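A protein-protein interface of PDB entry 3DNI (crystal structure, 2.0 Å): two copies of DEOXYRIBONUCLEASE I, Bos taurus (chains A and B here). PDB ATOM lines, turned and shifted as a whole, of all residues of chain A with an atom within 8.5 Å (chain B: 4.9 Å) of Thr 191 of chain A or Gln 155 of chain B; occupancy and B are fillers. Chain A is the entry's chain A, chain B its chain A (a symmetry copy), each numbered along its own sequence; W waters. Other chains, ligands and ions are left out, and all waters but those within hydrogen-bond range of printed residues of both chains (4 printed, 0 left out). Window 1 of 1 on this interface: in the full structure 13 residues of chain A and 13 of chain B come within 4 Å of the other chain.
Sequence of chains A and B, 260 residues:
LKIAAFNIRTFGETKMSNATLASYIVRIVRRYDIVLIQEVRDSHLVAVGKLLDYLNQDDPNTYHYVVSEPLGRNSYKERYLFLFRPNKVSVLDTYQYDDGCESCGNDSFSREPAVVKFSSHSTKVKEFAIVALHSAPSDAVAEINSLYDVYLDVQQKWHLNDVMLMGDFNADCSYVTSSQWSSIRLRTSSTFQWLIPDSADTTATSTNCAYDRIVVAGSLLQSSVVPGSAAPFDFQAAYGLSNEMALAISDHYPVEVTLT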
ATOM      1  N   TYR A 148       3.477  16.836  22.452  1.00  0.00           N
ATOM      2  CA  TYR A 148       2.988  16.540  21.034  1.00  0.00           C
ATOM      3  C   TYR A 148       1.468  16.654  21.065  1.00  0.00           C
ATOM      4  O   TYR A 148       0.890  17.245  20.136  1.00  0.00           O
ATOM      5  CB  TYR A 148       3.582  15.185  20.650  1.00  0.00           C
ATOM      6  CG  TYR A 148       3.074  14.685  19.315  1.00  0.00           C
ATOM      7  CD1 TYR A 148       3.733  15.134  18.165  1.00  0.00           C
ATOM      8  CD2 TYR A 148       1.945  13.899  19.200  1.00  0.00           C
ATOM      9  CE1 TYR A 148       3.277  14.699  16.882  1.00  0.00           C
ATOM     10  CE2 TYR A 148       1.474  13.495  17.932  1.00  0.00           C
ATOM     11  CZ  TYR A 148       2.176  13.868  16.803  1.00  0.00           C
ATOM     12  OH  TYR A 148       1.797  13.402  15.564  1.00  0.00           O
ATOM     13  N   TYR A 151       0.336  20.340  21.128  1.00  0.00           N
ATOM     14  CA  TYR A 151       0.395  20.961  19.752  1.00  0.00           C
ATOM     15  C   TYR A 151      -0.956  20.713  19.064  1.00  0.00           C
ATOM     16  O   TYR A 151      -1.670  21.677  18.543  1.00  0.00           O
ATOM     17  CB  TYR A 151       1.647  20.538  18.992  1.00  0.00           C
ATOM     18  CG  TYR A 151       1.783  21.119  17.607  1.00  0.00           C
ATOM     19  CD1 TYR A 151       2.046  22.491  17.435  1.00  0.00           C
ATOM     20  CD2 TYR A 151       1.538  20.366  16.477  1.00  0.00           C
ATOM     21  CE1 TYR A 151       2.167  23.045  16.132  1.00  0.00           C
ATOM     22  CE2 TYR A 151       1.574  20.916  15.175  1.00  0.00           C
ATOM     23  CZ  TYR A 151       1.921  22.243  15.010  1.00  0.00           C
ATOM     24  OH  TYR A 151       1.936  22.844  13.793  1.00  0.00           O
ATOM     25  N   GLN A 155      -3.843  23.261  17.591  1.00  0.00           N
ATOM     26  CA  GLN A 155      -4.247  23.219  16.171  1.00  0.00           C
ATOM     27  C   GLN A 155      -5.777  23.085  16.080  1.00  0.00           C
ATOM     28  O   GLN A 155      -6.359  23.704  15.179  1.00  0.00           O
ATOM     29  CB  GLN A 155      -3.637  22.125  15.305  1.00  0.00           C
ATOM     30  CG  GLN A 155      -2.145  22.184  15.077  1.00  0.00           C
ATOM     31  CD  GLN A 155      -1.731  21.008  14.215  1.00  0.00           C
ATOM     32  OE1 GLN A 155      -1.164  21.239  13.146  1.00  0.00           O
ATOM     33  NE2 GLN A 155      -2.048  19.813  14.678  1.00  0.00           N
ATOM     34  N   ASN A 161      -0.797  26.611  12.988  1.00  0.00           N
ATOM     35  CA  ASN A 161       0.319  25.632  12.913  1.00  0.00           C
ATOM     36  C   ASN A 161       1.545  26.287  13.552  1.00  0.00           C
ATOM     37  O   ASN A 161       2.354  25.482  13.984  1.00  0.00           O
ATOM     38  CB  ASN A 161       0.636  25.233  11.472  1.00  0.00           C
ATOM     39  CG  ASN A 161      -0.531  24.459  10.843  1.00  0.00           C
ATOM     40  OD1 ASN A 161      -0.625  24.564   9.566  1.00  0.00           O
ATOM     41  ND2 ASN A 161      -1.399  23.807  11.550  1.00  0.00           N
ATOM     42  N   ASP A 162       1.593  27.574  13.533  1.00  0.00           N
ATOM     43  CA  ASP A 162       2.738  28.356  14.084  1.00  0.00           C
ATOM     44  C   ASP A 162       2.812  28.379  15.610  1.00  0.00           C
ATOM     45  O   ASP A 162       2.080  29.240  16.142  1.00  0.00           O
ATOM     46  CB  ASP A 162       2.514  29.829  13.587  1.00  0.00           C
ATOM     47  CG  ASP A 162       2.683  29.834  12.082  1.00  0.00           C
ATOM     48  OD1 ASP A 162       3.804  29.418  11.802  1.00  0.00           O
ATOM     49  OD2 ASP A 162       1.769  30.215  11.364  1.00  0.00           O
ATOM     50  N   VAL A 163       3.494  27.504  16.242  1.00  0.00           N
ATOM     51  CA  VAL A 163       3.619  27.376  17.690  1.00  0.00           C
ATOM     52  C   VAL A 163       5.049  27.161  18.158  1.00  0.00           C
ATOM     53  O   VAL A 163       5.847  26.428  17.651  1.00  0.00           O
ATOM     54  CB  VAL A 163       2.738  26.213  18.153  1.00  0.00           C
ATOM     55  CG1 VAL A 163       2.775  25.953  19.670  1.00  0.00           C
ATOM     56  CG2 VAL A 163       1.301  26.384  17.636  1.00  0.00           C
ATOM     57  N   LEU A 165       7.170  26.155  21.462  1.00  0.00           N
ATOM     58  CA  LEU A 165       7.119  25.378  22.690  1.00  0.00           C
ATOM     59  C   LEU A 165       8.430  25.685  23.418  1.00  0.00           C
ATOM     60  O   LEU A 165       9.545  25.481  22.848  1.00  0.00           O
ATOM     61  CB  LEU A 165       6.841  23.886  22.397  1.00  0.00           C
ATOM     62  CG  LEU A 165       5.602  23.679  21.499  1.00  0.00           C
ATOM     63  CD1 LEU A 165       6.017  23.355  20.047  1.00  0.00           C
ATOM     64  CD2 LEU A 165       4.740  22.570  22.104  1.00  0.00           C
ATOM     65  N   ARG A 185       7.788  12.076  20.969  1.00  0.00           N
ATOM     66  CA  ARG A 185       7.166  12.412  19.690  1.00  0.00           C
ATOM     67  C   ARG A 185       7.467  13.815  19.226  1.00  0.00           C
ATOM     68  O   ARG A 185       7.430  14.135  18.014  1.00  0.00           O
ATOM     69  CB  ARG A 185       5.629  12.187  19.688  1.00  0.00           C
ATOM     70  CG  ARG A 185       5.326  10.651  19.683  1.00  0.00           C
ATOM     71  CD  ARG A 185       3.895  10.381  20.098  1.00  0.00           C
ATOM     72  NE  ARG A 185       3.556  11.167  21.284  1.00  0.00           N
ATOM     73  CZ  ARG A 185       2.346  11.513  21.674  1.00  0.00           C
ATOM     74  NH1 ARG A 185       1.205  11.180  21.001  1.00  0.00           N
ATOM     75  NH2 ARG A 185       2.216  12.155  22.866  1.00  0.00           N
ATOM     76  N   LEU A 186       7.723  14.666  20.259  1.00  0.00           N
ATOM     77  CA  LEU A 186       8.023  16.078  19.979  1.00  0.00           C
ATOM     78  C   LEU A 186       9.417  16.172  19.295  1.00  0.00           C
ATOM     79  O   LEU A 186       9.768  17.209  18.737  1.00  0.00           O
ATOM     80  CB  LEU A 186       7.979  16.926  21.289  1.00  0.00           C
ATOM     81  CG  LEU A 186       8.038  18.447  20.971  1.00  0.00           C
ATOM     82  CD1 LEU A 186       6.642  18.895  20.501  1.00  0.00           C
ATOM     83  CD2 LEU A 186       8.499  19.070  22.283  1.00  0.00           C
ATOM     84  N   ARG A 187      10.176  15.054  19.467  1.00  0.00           N
ATOM     85  CA  ARG A 187      11.494  15.007  18.848  1.00  0.00           C
ATOM     86  C   ARG A 187      11.510  14.151  17.565  1.00  0.00           C
ATOM     87  O   ARG A 187      12.195  14.543  16.590  1.00  0.00           O
ATOM     88  CB  ARG A 187      12.570  14.499  19.808  1.00  0.00           C
ATOM     89  CG  ARG A 187      13.996  14.720  19.274  1.00  0.00           C
ATOM     90  CD  ARG A 187      14.384  16.122  19.463  1.00  0.00           C
ATOM     91  NE  ARG A 187      15.726  16.459  19.071  1.00  0.00           N
ATOM     92  CZ  ARG A 187      16.743  16.686  19.888  1.00  0.00           C
ATOM     93  NH1 ARG A 187      16.699  16.656  21.188  1.00  0.00           N
ATOM     94  NH2 ARG A 187      17.934  16.941  19.294  1.00  0.00           N
ATOM     95  N   THR A 188      10.779  13.022  17.603  1.00  0.00           N
ATOM     96  CA  THR A 188      10.875  12.131  16.420  1.00  0.00           C
ATOM     97  C   THR A 188      10.047  12.624  15.254  1.00  0.00           C
ATOM     98  O   THR A 188      10.310  12.277  14.093  1.00  0.00           O
ATOM     99  CB  THR A 188      10.573  10.667  16.879  1.00  0.00           C
ATOM    100  OG1 THR A 188       9.223  10.712  17.396  1.00  0.00           O
ATOM    101  CG2 THR A 188      11.538  10.144  17.961  1.00  0.00           C
ATOM    102  N   SER A 189       9.038  13.442  15.583  1.00  0.00           N
ATOM    103  CA  SER A 189       8.232  14.067  14.515  1.00  0.00           C
ATOM    104  C   SER A 189       9.008  15.248  13.964  1.00  0.00           C
ATOM    105  O   SER A 189       9.511  16.122  14.664  1.00  0.00           O
ATOM    106  CB  SER A 189       6.834  14.408  15.051  1.00  0.00           C
ATOM    107  OG  SER A 189       6.379  15.251  14.036  1.00  0.00           O
ATOM    108  N   SER A 190       9.225  15.272  12.631  1.00  0.00           N
ATOM    109  CA  SER A 190       9.933  16.277  11.877  1.00  0.00           C
ATOM    110  C   SER A 190       9.075  17.548  11.693  1.00  0.00           C
ATOM    111  O   SER A 190       9.487  18.486  11.022  1.00  0.00           O
ATOM    112  CB  SER A 190      10.496  15.797  10.509  1.00  0.00           C
ATOM    113  OG  SER A 190       9.525  14.908   9.959  1.00  0.00           O
ATOM    114  N   THR A 191       7.917  17.568  12.319  1.00  0.00           N
ATOM    115  CA  THR A 191       7.063  18.759  12.266  1.00  0.00           C
ATOM    116  C   THR A 191       7.802  19.922  13.021  1.00  0.00           C
ATOM    117  O   THR A 191       7.619  21.121  12.837  1.00  0.00           O
ATOM    118  CB  THR A 191       5.658  18.580  12.890  1.00  0.00           C
ATOM    119  OG1 THR A 191       4.930  17.548  12.057  1.00  0.00           O
ATOM    120  CG2 THR A 191       4.694  19.787  12.998  1.00  0.00           C
ATOM    121  N   PHE A 192       8.559  19.492  14.012  1.00  0.00           N
ATOM    122  CA  PHE A 192       9.249  20.348  14.987  1.00  0.00           C
ATOM    123  C   PHE A 192      10.719  20.512  14.797  1.00  0.00           C
ATOM    124  O   PHE A 192      11.438  19.555  14.548  1.00  0.00           O
ATOM    125  CB  PHE A 192       8.979  19.797  16.452  1.00  0.00           C
ATOM    126  CG  PHE A 192       7.506  19.502  16.656  1.00  0.00           C
ATOM    127  CD1 PHE A 192       6.651  20.543  17.054  1.00  0.00           C
ATOM    128  CD2 PHE A 192       7.026  18.203  16.549  1.00  0.00           C
ATOM    129  CE1 PHE A 192       5.296  20.266  17.239  1.00  0.00           C
ATOM    130  CE2 PHE A 192       5.679  17.918  16.714  1.00  0.00           C
ATOM    131  CZ  PHE A 192       4.767  18.946  17.018  1.00  0.00           C
ATOM    132  N   GLN A 193      11.172  21.746  14.999  1.00  0.00           N
ATOM    133  CA  GLN A 193      12.613  22.082  14.913  1.00  0.00           C
ATOM    134  C   GLN A 193      13.076  22.486  16.319  1.00  0.00           C
ATOM    135  O   GLN A 193      12.410  23.367  16.897  1.00  0.00           O
ATOM    136  CB  GLN A 193      12.750  23.267  13.997  1.00  0.00           C
ATOM    137  CG  GLN A 193      14.105  23.829  13.643  1.00  0.00           C
ATOM    138  CD  GLN A 193      13.851  24.516  12.277  1.00  0.00           C
ATOM    139  OE1 GLN A 193      13.903  25.703  12.138  1.00  0.00           O
ATOM    140  NE2 GLN A 193      13.436  23.666  11.285  1.00  0.00           N
ATOM    141  N   TRP A 194      14.162  21.873  16.729  1.00  0.00           N
ATOM    142  CA  TRP A 194      14.723  22.182  18.080  1.00  0.00           C
ATOM    143  C   TRP A 194      15.808  23.218  17.899  1.00  0.00           C
ATOM    144  O   TRP A 194      16.922  22.910  17.329  1.00  0.00           O
ATOM    145  CB  TRP A 194      15.219  20.831  18.672  1.00  0.00           C
ATOM    146  CG  TRP A 194      14.084  19.937  19.101  1.00  0.00           C
ATOM    147  CD1 TRP A 194      13.136  19.343  18.303  1.00  0.00           C
ATOM    148  CD2 TRP A 194      13.761  19.588  20.451  1.00  0.00           C
ATOM    149  NE1 TRP A 194      12.290  18.616  19.088  1.00  0.00           N
ATOM    150  CE2 TRP A 194      12.622  18.752  20.408  1.00  0.00           C
ATOM    151  CE3 TRP A 194      14.355  19.856  21.685  1.00  0.00           C
ATOM    152  CZ2 TRP A 194      12.085  18.208  21.541  1.00  0.00           C
ATOM    153  CZ3 TRP A 194      13.822  19.343  22.853  1.00  0.00           C
ATOM    154  CH2 TRP A 194      12.675  18.501  22.763  1.00  0.00           C
ATOM    155  N   VAL A 215      11.440  24.996  20.846  1.00  0.00           N
ATOM    156  CA  VAL A 215      10.968  24.168  19.744  1.00  0.00           C
ATOM    157  C   VAL A 215       9.983  24.990  18.913  1.00  0.00           C
ATOM    158  O   VAL A 215       9.150  25.674  19.570  1.00  0.00           O
ATOM    159  CB  VAL A 215      10.267  22.892  20.279  1.00  0.00           C
ATOM    160  CG1 VAL A 215       9.868  21.824  19.238  1.00  0.00           C
ATOM    161  CG2 VAL A 215      11.113  22.186  21.335  1.00  0.00           C
ATOM    162  N   VAL A 216       9.976  24.884  17.580  1.00  0.00           N
ATOM    163  CA  VAL A 216       9.004  25.651  16.767  1.00  0.00           C
ATOM    164  C   VAL A 216       8.435  24.657  15.721  1.00  0.00           C
ATOM    165  O   VAL A 216       9.231  23.846  15.218  1.00  0.00           O
ATOM    166  CB  VAL A 216       9.600  26.881  16.085  1.00  0.00           C
ATOM    167  CG1 VAL A 216       9.731  28.126  17.039  1.00  0.00           C
ATOM    168  CG2 VAL A 216      10.998  26.692  15.488  1.00  0.00           C
ATOM    169  N   ALA A 217       7.202  24.894  15.407  1.00  0.00           N
ATOM    170  CA  ALA A 217       6.416  24.189  14.435  1.00  0.00           C
ATOM    171  C   ALA A 217       5.740  25.325  13.624  1.00  0.00           C
ATOM    172  O   ALA A 217       5.544  26.415  14.233  1.00  0.00           O
ATOM    173  CB  ALA A 217       5.397  23.287  15.105  1.00  0.00           C
ATOM    174  N   GLY A 218       5.510  25.053  12.344  1.00  0.00           N
ATOM    175  CA  GLY A 218       4.875  26.082  11.461  1.00  0.00           C
ATOM    176  C   GLY A 218       5.881  26.590  10.466  1.00  0.00           C
ATOM    177  O   GLY A 218       6.832  27.225  10.887  1.00  0.00           O
ATOM    178  N   SER A 219       5.682  26.511   9.134  1.00  0.00           N
ATOM    179  CA  SER A 219       6.711  27.054   8.214  1.00  0.00           C
ATOM    180  C   SER A 219       6.816  28.585   8.318  1.00  0.00           C
ATOM    181  O   SER A 219       7.918  29.111   8.163  1.00  0.00           O
ATOM    182  CB  SER A 219       6.512  26.567   6.777  1.00  0.00           C
ATOM    183  OG  SER A 219       5.095  26.385   6.706  1.00  0.00           O
ATOM    184  N   GLN A 222       8.873  29.137  11.463  1.00  0.00           N
ATOM    185  CA  GLN A 222      10.225  28.623  11.187  1.00  0.00           C
ATOM    186  C   GLN A 222      10.925  29.597  10.233  1.00  0.00           C
ATOM    187  O   GLN A 222      12.153  29.839  10.452  1.00  0.00           O
ATOM    188  CB  GLN A 222      10.248  27.165  10.769  1.00  0.00           C
ATOM    189  CG  GLN A 222      10.025  26.139  11.882  1.00  0.00           C
ATOM    190  CD  GLN A 222       9.749  24.742  11.352  1.00  0.00           C
ATOM    191  OE1 GLN A 222       9.764  24.612  10.123  1.00  0.00           O
ATOM    192  NE2 GLN A 222       9.515  23.691  12.135  1.00  0.00           N
ATOM    193  N   TYR B 151       0.604   9.091   9.534  1.00  0.00           N
ATOM    194  CA  TYR B 151       1.475  10.275   9.181  1.00  0.00           C
ATOM    195  C   TYR B 151       2.692  10.263  10.118  1.00  0.00           C
ATOM    196  O   TYR B 151       3.922  10.302   9.677  1.00  0.00           O
ATOM    197  CB  TYR B 151       0.670  11.567   9.107  1.00  0.00           C
ATOM    198  CG  TYR B 151       1.467  12.799   8.755  1.00  0.00           C
ATOM    199  CD1 TYR B 151       1.992  12.959   7.459  1.00  0.00           C
ATOM    200  CD2 TYR B 151       1.807  13.739   9.706  1.00  0.00           C
ATOM    201  CE1 TYR B 151       2.750  14.113   7.125  1.00  0.00           C
ATOM    202  CE2 TYR B 151       2.628  14.853   9.413  1.00  0.00           C
ATOM    203  CZ  TYR B 151       3.065  15.049   8.119  1.00  0.00           C
ATOM    204  OH  TYR B 151       3.888  16.074   7.777  1.00  0.00           O
ATOM    205  N   LEU B 152       2.423  10.210  11.417  1.00  0.00           N
ATOM    206  CA  LEU B 152       3.459  10.185  12.422  1.00  0.00           C
ATOM    207  C   LEU B 152       4.482   9.091  12.133  1.00  0.00           C
ATOM    208  O   LEU B 152       5.715   9.305  12.232  1.00  0.00           O
ATOM    209  CB  LEU B 152       2.886  10.138  13.868  1.00  0.00           C
ATOM    210  CG  LEU B 152       3.989   9.984  14.958  1.00  0.00           C
ATOM    211  CD1 LEU B 152       5.077  11.051  14.963  1.00  0.00           C
ATOM    212  CD2 LEU B 152       3.314   9.969  16.324  1.00  0.00           C
ATOM    213  N   ASP B 153       3.919   7.917  11.791  1.00  0.00           N
ATOM    214  CA  ASP B 153       4.827   6.757  11.559  1.00  0.00           C
ATOM    215  C   ASP B 153       5.764   7.007  10.402  1.00  0.00           C
ATOM    216  O   ASP B 153       6.941   6.592  10.448  1.00  0.00           O
ATOM    217  CB  ASP B 153       3.917   5.518  11.471  1.00  0.00           C
ATOM    218  CG  ASP B 153       4.886   4.317  11.432  1.00  0.00           C
ATOM    219  OD1 ASP B 153       5.399   3.908  12.414  1.00  0.00           O
ATOM    220  OD2 ASP B 153       5.125   3.942  10.287  1.00  0.00           O
ATOM    221  N   VAL B 154       5.273   7.648   9.376  1.00  0.00           N
ATOM    222  CA  VAL B 154       6.039   8.030   8.206  1.00  0.00           C
ATOM    223  C   VAL B 154       7.131   9.038   8.591  1.00  0.00           C
ATOM    224  O   VAL B 154       8.261   8.955   8.095  1.00  0.00           O
ATOM    225  CB  VAL B 154       5.114   8.634   7.103  1.00  0.00           C
ATOM    226  CG1 VAL B 154       5.904   9.341   6.005  1.00  0.00           C
ATOM    227  CG2 VAL B 154       4.251   7.512   6.561  1.00  0.00           C
ATOM    228  N   GLN B 155       6.745   9.981   9.419  1.00  0.00           N
ATOM    229  CA  GLN B 155       7.672  11.041   9.863  1.00  0.00           C
ATOM    230  C   GLN B 155       8.810  10.410  10.687  1.00  0.00           C
ATOM    231  O   GLN B 155       9.949  10.875  10.549  1.00  0.00           O
ATOM    232  CB  GLN B 155       7.086  12.180  10.686  1.00  0.00           C
ATOM    233  CG  GLN B 155       6.087  13.078   9.996  1.00  0.00           C
ATOM    234  CD  GLN B 155       5.608  14.129  10.978  1.00  0.00           C
ATOM    235  OE1 GLN B 155       5.771  15.316  10.689  1.00  0.00           O
ATOM    236  NE2 GLN B 155       5.076  13.674  12.097  1.00  0.00           N
ATOM    237  N   GLN B 156       8.443   9.429  11.471  1.00  0.00           N
ATOM    238  CA  GLN B 156       9.452   8.777  12.342  1.00  0.00           C
ATOM    239  C   GLN B 156      10.420   7.917  11.549  1.00  0.00           C
ATOM    240  O   GLN B 156      11.585   7.826  11.920  1.00  0.00           O
ATOM    241  CB  GLN B 156       8.786   7.962  13.445  1.00  0.00           C
ATOM    242  CG  GLN B 156       8.223   8.802  14.534  1.00  0.00           C
ATOM    243  CD  GLN B 156       7.431   8.082  15.584  1.00  0.00           C
ATOM    244  OE1 GLN B 156       7.449   8.625  16.720  1.00  0.00           O
ATOM    245  NE2 GLN B 156       6.809   6.955  15.268  1.00  0.00           N
ATOM    246  N   LYS B 157       9.930   7.301  10.483  1.00  0.00           N
ATOM    247  CA  LYS B 157      10.682   6.412   9.611  1.00  0.00           C
ATOM    248  C   LYS B 157      11.519   7.087   8.564  1.00  0.00           C
ATOM    249  O   LYS B 157      12.716   6.729   8.470  1.00  0.00           O
ATOM    250  CB  LYS B 157       9.721   5.373   8.925  1.00  0.00           C
ATOM    251  CG  LYS B 157       9.426   4.316   9.985  1.00  0.00           C
ATOM    252  CD  LYS B 157       8.627   3.111   9.600  1.00  0.00           C
ATOM    253  CE  LYS B 157       9.006   2.401   8.360  1.00  0.00           C
ATOM    254  NZ  LYS B 157      10.392   1.811   8.354  1.00  0.00           N
ATOM    255  N   TRP B 158      10.899   7.969   7.782  1.00  0.00           N
ATOM    256  CA  TRP B 158      11.639   8.642   6.688  1.00  0.00           C
ATOM    257  C   TRP B 158      12.022  10.085   7.027  1.00  0.00           C
ATOM    258  O   TRP B 158      12.862  10.631   6.305  1.00  0.00           O
ATOM    259  CB  TRP B 158      10.875   8.541   5.385  1.00  0.00           C
ATOM    260  CG  TRP B 158      10.723   7.122   4.872  1.00  0.00           C
ATOM    261  CD1 TRP B 158      11.628   6.096   4.965  1.00  0.00           C
ATOM    262  CD2 TRP B 158       9.603   6.606   4.181  1.00  0.00           C
ATOM    263  NE1 TRP B 158      11.115   4.974   4.348  1.00  0.00           N
ATOM    264  CE2 TRP B 158       9.885   5.258   3.858  1.00  0.00           C
ATOM    265  CE3 TRP B 158       8.376   7.148   3.817  1.00  0.00           C
ATOM    266  CZ2 TRP B 158       8.993   4.436   3.222  1.00  0.00           C
ATOM    267  CZ3 TRP B 158       7.473   6.360   3.136  1.00  0.00           C
ATOM    268  CH2 TRP B 158       7.774   5.020   2.847  1.00  0.00           C
ATOM    269  N   HIS B 159      11.462  10.607   8.110  1.00  0.00           N
ATOM    270  CA  HIS B 159      11.843  11.992   8.482  1.00  0.00           C
ATOM    271  C   HIS B 159      11.347  12.940   7.410  1.00  0.00           C
ATOM    272  O   HIS B 159      11.928  14.023   7.134  1.00  0.00           O
ATOM    273  CB  HIS B 159      13.356  12.092   8.679  1.00  0.00           C
ATOM    274  CG  HIS B 159      13.869  10.998   9.607  1.00  0.00           C
ATOM    275  ND1 HIS B 159      13.690  10.993  10.954  1.00  0.00           N
ATOM    276  CD2 HIS B 159      14.631   9.910   9.296  1.00  0.00           C
ATOM    277  CE1 HIS B 159      14.294   9.929  11.454  1.00  0.00           C
ATOM    278  NE2 HIS B 159      14.896   9.262  10.465  1.00  0.00           N
ATOM    279  N   LEU B 160      10.214  12.565   6.825  1.00  0.00           N
ATOM    280  CA  LEU B 160       9.661  13.372   5.745  1.00  0.00           C
ATOM    281  C   LEU B 160       8.349  13.949   6.177  1.00  0.00           C
ATOM    282  O   LEU B 160       7.515  13.187   6.745  1.00  0.00           O
ATOM    283  CB  LEU B 160       9.618  12.333   4.571  1.00  0.00           C
ATOM    284  CG  LEU B 160       9.280  12.932   3.228  1.00  0.00           C
ATOM    285  CD1 LEU B 160      10.527  13.194   2.435  1.00  0.00           C
ATOM    286  CD2 LEU B 160       8.436  11.840   2.524  1.00  0.00           C
ATOM    287  N   ASN B 161       8.096  15.177   5.832  1.00  0.00           N
ATOM    288  CA  ASN B 161       6.823  15.851   6.199  1.00  0.00           C
ATOM    289  C   ASN B 161       5.915  15.813   4.969  1.00  0.00           C
ATOM    290  O   ASN B 161       4.728  15.883   5.242  1.00  0.00           O
ATOM    291  CB  ASN B 161       7.046  17.299   6.635  1.00  0.00           C
ATOM    292  CG  ASN B 161       7.850  17.366   7.942  1.00  0.00           C
ATOM    293  OD1 ASN B 161       8.547  18.434   8.094  1.00  0.00           O
ATOM    294  ND2 ASN B 161       7.880  16.391   8.793  1.00  0.00           N
HETATM  295  O   HOH W   1       4.467  18.220   9.277  1.00  0.00           O
HETATM  296  O   HOH W   2       8.843   8.715  19.593  1.00  0.00           O
HETATM  297  O   HOH W   3      11.951  12.759  11.787  1.00  0.00           O
HETATM  298  O   HOH W   4       2.888  13.743  13.263  1.00  0.00           O
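Among the printed residues, merely in contact across the chains: Ser 190 of chain A with His 159 of chain B (3.7 Å), Thr 191 of chain A with Asn 161 of chain B (3.7 Å), Ser 190 of chain A with Gln 155 of chain B (3.7 Å), Ser 189 of chain A with Leu 152 of chain B (3.8 Å), Thr 188 of chain A with Gln 155 of chain B (3.8 Å), Tyr 148 of chain A with Leu 152 of chain B (3.8 Å), Arg 185 of chain A with Leu 152 of chain B (3.8 Å) and Ser 190 of chain A with Leu 160 of chain B (3.97 Å).
3 positions are printed for both chains.
Of the printed residues of chain B, Thr 188 of chain A touches Gln 155 (3.8 Å) and Gln 156 (2.8 Å). Thr 191 of chain A touches just these residues of chain B: Gln 155 and Asn 161. Of the printed residues of chain A, Leu 152 of chain B touches Tyr 148 (3.8 Å), Arg 185 (3.8 Å) and Ser 189 (3.8 Å). Gln 155 of chain B touches four residues of chain A. The nearest residue of chain B that does not touch Thr 191 of chain A is Tyr 151 of chain B (4.4 Å).
Water W4 bridges NE2 of Gln 155 of chain B and OH of Tyr 148 of chain A. Water W3 lies within hydrogen-bond range of a ring nitrogen (ND1) of His 159 of chain B, the backbone carbonyl oxygen (O) of Thr 188 of chain A and the backbone carbonyl oxygen (O) of Gln 155 of chain B. Water W1 lies within hydrogen-bond range of the side-chain hydroxyl of Tyr 151 of chain B, the side-chain hydroxyl of Thr 191 of chain A and the side-chain amide oxygen of Gln 155 of chain B. Water W2 lies within hydrogen-bond range of the side-chain hydroxyl of Thr 188 of chain A (3.0 Å) and the side-chain amide oxygen of Gln 156 of chain B (3.2 Å).
Of the 11 printed residues of chain B, 6 touch a printed residue of chain A. Hydrophobic or aromatic side chains of chain B that line the printed part of chain A: Leu 152. Among the printed residues, no Asp or Glu carboxylate lies within 4 Å of a Lys or Arg side-chain nitrogen of the other chain.
The side-chain hydroxyl of Ser 189 of chain A sits close to the backbone NH of Thr 191 of chain A, at 3.3 Å. The backbone carbonyl oxygen of Thr 191 of chain A lies within hydrogen-bond range of the side-chain amide nitrogen of Gln 222 of chain A (3.3 Å). The backbone carbonyl oxygen of Asn 161 of chain B lies within hydrogen-bond range of the side-chain hydroxyl of Tyr 151 of chain B. The side-chain amide oxygen (OE1) of Gln 155 of chain B is in hydrogen-bond range of the side-chain amide nitrogen (ND2) of Asn 161 of chain B (3.0 Å).
OG1 of Thr 188 of chain A sits at hydrogen-bond distance from OE1 of Gln 156 of chain B. The side-chain amide nitrogen (NE2) of Gln 155 of chain B lies within hydrogen-bond range of the side-chain hydroxyl (OG) of Ser 189 of chain A. The side-chain amide nitrogen (ND2) of Asn 161 of chain B sits at hydrogen-bond distance from the side-chain hydroxyl (OG) of Ser 190 of chain A (2.5 Å). The side-chain hydroxyl of Thr 191 of chain A lies within hydrogen-bond range of the side-chain amide oxygen of Gln 155 of chain B (2.7 Å).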
